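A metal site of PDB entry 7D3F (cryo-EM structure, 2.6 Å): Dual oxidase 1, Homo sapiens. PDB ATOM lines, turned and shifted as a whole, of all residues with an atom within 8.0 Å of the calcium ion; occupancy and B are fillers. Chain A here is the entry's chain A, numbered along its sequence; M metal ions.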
ATOM      1  N   PHE A 860       2.263 -14.940 -21.694  1.00  0.00           N
ATOM      2  CA  PHE A 860       2.989 -15.280 -20.473  1.00  0.00           C
ATOM      3  C   PHE A 860       4.239 -14.412 -20.321  1.00  0.00           C
ATOM      4  O   PHE A 860       4.555 -13.953 -19.224  1.00  0.00           O
ATOM      5  CB  PHE A 860       3.360 -16.762 -20.474  1.00  0.00           C
ATOM      6  CG  PHE A 860       4.053 -17.226 -19.229  1.00  0.00           C
ATOM      7  CD1 PHE A 860       5.435 -17.257 -19.155  1.00  0.00           C
ATOM      8  CD2 PHE A 860       3.321 -17.641 -18.129  1.00  0.00           C
ATOM      9  CE1 PHE A 860       6.071 -17.682 -18.002  1.00  0.00           C
ATOM     10  CE2 PHE A 860       3.947 -18.068 -16.976  1.00  0.00           C
ATOM     11  CZ  PHE A 860       5.326 -18.084 -16.916  1.00  0.00           C
ATOM     12  N   ARG A 861       4.952 -14.177 -21.427  1.00  0.00           N
ATOM     13  CA  ARG A 861       6.140 -13.337 -21.377  1.00  0.00           C
ATOM     14  C   ARG A 861       5.786 -11.886 -21.064  1.00  0.00           C
ATOM     15  O   ARG A 861       6.554 -11.188 -20.393  1.00  0.00           O
ATOM     16  CB  ARG A 861       6.895 -13.422 -22.702  1.00  0.00           C
ATOM     17  CG  ARG A 861       7.579 -14.759 -22.938  1.00  0.00           C
ATOM     18  CD  ARG A 861       8.269 -14.779 -24.299  1.00  0.00           C
ATOM     19  NE  ARG A 861       9.025 -13.548 -24.541  1.00  0.00           N
ATOM     20  CZ  ARG A 861      10.250 -13.318 -24.068  1.00  0.00           C
ATOM     21  NH1 ARG A 861      10.850 -14.231 -23.319  1.00  0.00           N
ATOM     22  NH2 ARG A 861      10.864 -12.178 -24.345  1.00  0.00           N
ATOM     23  N   TYR A 863       3.125 -10.940 -19.289  1.00  0.00           N
ATOM     24  CA  TYR A 863       2.436 -10.824 -18.003  1.00  0.00           C
ATOM     25  C   TYR A 863       3.412 -10.690 -16.839  1.00  0.00           C
ATOM     26  O   TYR A 863       3.156  -9.919 -15.898  1.00  0.00           O
ATOM     27  CB  TYR A 863       1.517 -12.013 -17.786  1.00  0.00           C
ATOM     28  N   ASP A 864       4.522 -11.422 -16.863  1.00  0.00           N
ATOM     29  CA  ASP A 864       5.434 -11.491 -15.721  1.00  0.00           C
ATOM     30  C   ASP A 864       6.428 -10.339 -15.774  1.00  0.00           C
ATOM     31  O   ASP A 864       7.144 -10.177 -16.768  1.00  0.00           O
ATOM     32  CB  ASP A 864       6.150 -12.834 -15.680  1.00  0.00           C
ATOM     33  CG  ASP A 864       6.717 -13.246 -17.027  1.00  0.00           C
ATOM     34  OD1 ASP A 864       6.533 -12.499 -18.002  1.00  0.00           O
ATOM     35  OD2 ASP A 864       7.344 -14.324 -17.102  1.00  0.00           O
ATOM     36  N   PHE A 865       6.457  -9.532 -14.711  1.00  0.00           N
ATOM     37  CA  PHE A 865       7.407  -8.429 -14.646  1.00  0.00           C
ATOM     38  C   PHE A 865       8.829  -8.938 -14.521  1.00  0.00           C
ATOM     39  O   PHE A 865       9.728  -8.499 -15.254  1.00  0.00           O
ATOM     40  CB  PHE A 865       7.046  -7.507 -13.471  1.00  0.00           C
ATOM     41  CG  PHE A 865       7.605  -6.114 -13.594  1.00  0.00           C
ATOM     42  CD1 PHE A 865       7.357  -5.168 -12.606  1.00  0.00           C
ATOM     43  CD2 PHE A 865       8.356  -5.732 -14.701  1.00  0.00           C
ATOM     44  CE1 PHE A 865       7.860  -3.884 -12.712  1.00  0.00           C
ATOM     45  CE2 PHE A 865       8.858  -4.448 -14.807  1.00  0.00           C
ATOM     46  CZ  PHE A 865       8.605  -3.525 -13.813  1.00  0.00           C
ATOM     47  N   ASP A 866       9.066  -9.860 -13.591  1.00  0.00           N
ATOM     48  CA  ASP A 866      10.413 -10.374 -13.382  1.00  0.00           C
ATOM     49  C   ASP A 866      10.839 -11.311 -14.514  1.00  0.00           C
ATOM     50  O   ASP A 866      12.027 -11.371 -14.850  1.00  0.00           O
ATOM     51  CB  ASP A 866      10.509 -11.106 -12.041  1.00  0.00           C
ATOM     52  CG  ASP A 866       9.492 -12.221 -11.902  1.00  0.00           C
ATOM     53  OD1 ASP A 866       8.615 -12.339 -12.780  1.00  0.00           O
ATOM     54  OD2 ASP A 866       9.577 -12.985 -10.923  1.00  0.00           O
ATOM     55  N   GLY A 867       9.888 -12.025 -15.120  1.00  0.00           N
ATOM     56  CA  GLY A 867      10.214 -12.944 -16.183  1.00  0.00           C
ATOM     57  C   GLY A 867      11.054 -14.127 -15.759  1.00  0.00           C
ATOM     58  O   GLY A 867      12.006 -14.483 -16.464  1.00  0.00           O
ATOM     59  N   ASN A 868      10.737 -14.734 -14.624  1.00  0.00           N
ATOM     60  CA  ASN A 868      11.482 -15.877 -14.111  1.00  0.00           C
ATOM     61  C   ASN A 868      10.866 -17.214 -14.497  1.00  0.00           C
ATOM     62  O   ASN A 868      11.211 -18.242 -13.914  1.00  0.00           O
ATOM     63  CB  ASN A 868      11.602 -15.785 -12.583  1.00  0.00           C
ATOM     64  CG  ASN A 868      10.271 -15.955 -11.876  1.00  0.00           C
ATOM     65  OD1 ASN A 868       9.224 -15.582 -12.405  1.00  0.00           O
ATOM     66  ND2 ASN A 868      10.308 -16.509 -10.673  1.00  0.00           N
ATOM     67  N   GLY A 869       9.954 -17.214 -15.465  1.00  0.00           N
ATOM     68  CA  GLY A 869       9.310 -18.426 -15.920  1.00  0.00           C
ATOM     69  C   GLY A 869       8.088 -18.855 -15.124  1.00  0.00           C
ATOM     70  O   GLY A 869       7.513 -19.901 -15.438  1.00  0.00           O
ATOM     71  N   LEU A 870       7.686 -18.084 -14.124  1.00  0.00           N
ATOM     72  CA  LEU A 870       6.508 -18.394 -13.331  1.00  0.00           C
ATOM     73  C   LEU A 870       5.817 -17.098 -12.933  1.00  0.00           C
ATOM     74  O   LEU A 870       6.428 -16.031 -12.894  1.00  0.00           O
ATOM     75  CB  LEU A 870       6.860 -19.201 -12.076  1.00  0.00           C
ATOM     76  N   ILE A 871       4.517 -17.208 -12.648  1.00  0.00           N
ATOM     77  CA  ILE A 871       3.690 -16.067 -12.279  1.00  0.00           C
ATOM     78  C   ILE A 871       3.349 -16.193 -10.806  1.00  0.00           C
ATOM     79  O   ILE A 871       2.723 -17.171 -10.391  1.00  0.00           O
ATOM     80  CB  ILE A 871       2.425 -15.979 -13.141  1.00  0.00           C
ATOM     81  N   SER A 872       3.742 -15.185 -10.018  1.00  0.00           N
ATOM     82  CA  SER A 872       3.413 -15.176  -8.611  1.00  0.00           C
ATOM     83  C   SER A 872       1.949 -14.800  -8.402  1.00  0.00           C
ATOM     84  O   SER A 872       1.324 -14.161  -9.252  1.00  0.00           O
ATOM     85  CB  SER A 872       4.316 -14.193  -7.851  1.00  0.00           C
ATOM     86  OG  SER A 872       3.907 -14.056  -6.500  1.00  0.00           O
ATOM     87  N   GLU A 875       1.939 -11.287  -8.307  1.00  0.00           N
ATOM     88  CA  GLU A 875       2.188 -10.836  -9.674  1.00  0.00           C
ATOM     89  C   GLU A 875       0.987 -11.102 -10.579  1.00  0.00           C
ATOM     90  O   GLU A 875       0.658 -10.276 -11.429  1.00  0.00           O
ATOM     91  CB  GLU A 875       3.439 -11.524 -10.216  1.00  0.00           C
ATOM     92  CG  GLU A 875       3.763 -11.200 -11.656  1.00  0.00           C
ATOM     93  CD  GLU A 875       5.052 -11.845 -12.118  1.00  0.00           C
ATOM     94  OE1 GLU A 875       6.136 -11.303 -11.803  1.00  0.00           O
ATOM     95  OE2 GLU A 875       4.988 -12.915 -12.765  1.00  0.00           O
ATOM     96  N   GLU A 914       2.886 -21.963  -7.680  1.00  0.00           N
ATOM     97  CA  GLU A 914       2.683 -20.951  -8.712  1.00  0.00           C
ATOM     98  C   GLU A 914       1.993 -21.547  -9.930  1.00  0.00           C
ATOM     99  O   GLU A 914       1.632 -22.716  -9.937  1.00  0.00           O
ATOM    100  CB  GLU A 914       4.020 -20.328  -9.117  1.00  0.00           C
ATOM    101  CG  GLU A 914       4.877 -19.865  -7.941  1.00  0.00           C
ATOM    102  CD  GLU A 914       4.447 -18.518  -7.385  1.00  0.00           C
ATOM    103  OE1 GLU A 914       5.231 -17.552  -7.513  1.00  0.00           O
ATOM    104  OE2 GLU A 914       3.336 -18.422  -6.827  1.00  0.00           O
ATOM    105  N   LEU A 915       1.814 -20.725 -10.960  1.00  0.00           N
ATOM    106  CA  LEU A 915       1.208 -21.148 -12.220  1.00  0.00           C
ATOM    107  C   LEU A 915       2.241 -20.961 -13.325  1.00  0.00           C
ATOM    108  O   LEU A 915       2.513 -19.834 -13.746  1.00  0.00           O
ATOM    109  CB  LEU A 915      -0.069 -20.355 -12.518  1.00  0.00           C
HETATM  110 CA    CA M   1       7.889 -14.381 -14.066  1.00  0.00          CA
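The calcium ion is bound by OD1 of Asn 868 (2.4 Å).
The backbone carbonyl oxygen (O) of Leu 870 is bound to the calcium ion (2.5 Å).
OD1 of Asp 866 binds the calcium ion (2.5 Å).
Slightly farther from the calcium ion lies N of Asn 868 (2.9 Å).
Slightly farther from the calcium ion lies OD2 of Asp 864 (3.1 Å).
O of Phe 860 sits close to OD1 of Asp 864 (2.7 Å).
The side-chain carboxylate of Asp 864 lies close to the backbone carbonyl oxygen of Arg 861 (2.7 Å).
The side-chain carboxylate (OE1) of Glu 875 is in hydrogen-bond range of the backbone NH (N) of Phe 865 (3.4 Å).
Gly 867 touches the calcium ion.
Gly 869 touches the calcium ion (N to CA, 3.8 Å).
Glu 875 touches the calcium ion.
Within 4 Å of the calcium ion: Asp 864, Asp 866, Gly 867, Asn 868, Gly 869, Leu 870 and Glu 875.
Along chain A the residues within 4 Å of the calcium ion span positions 864 to 875.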
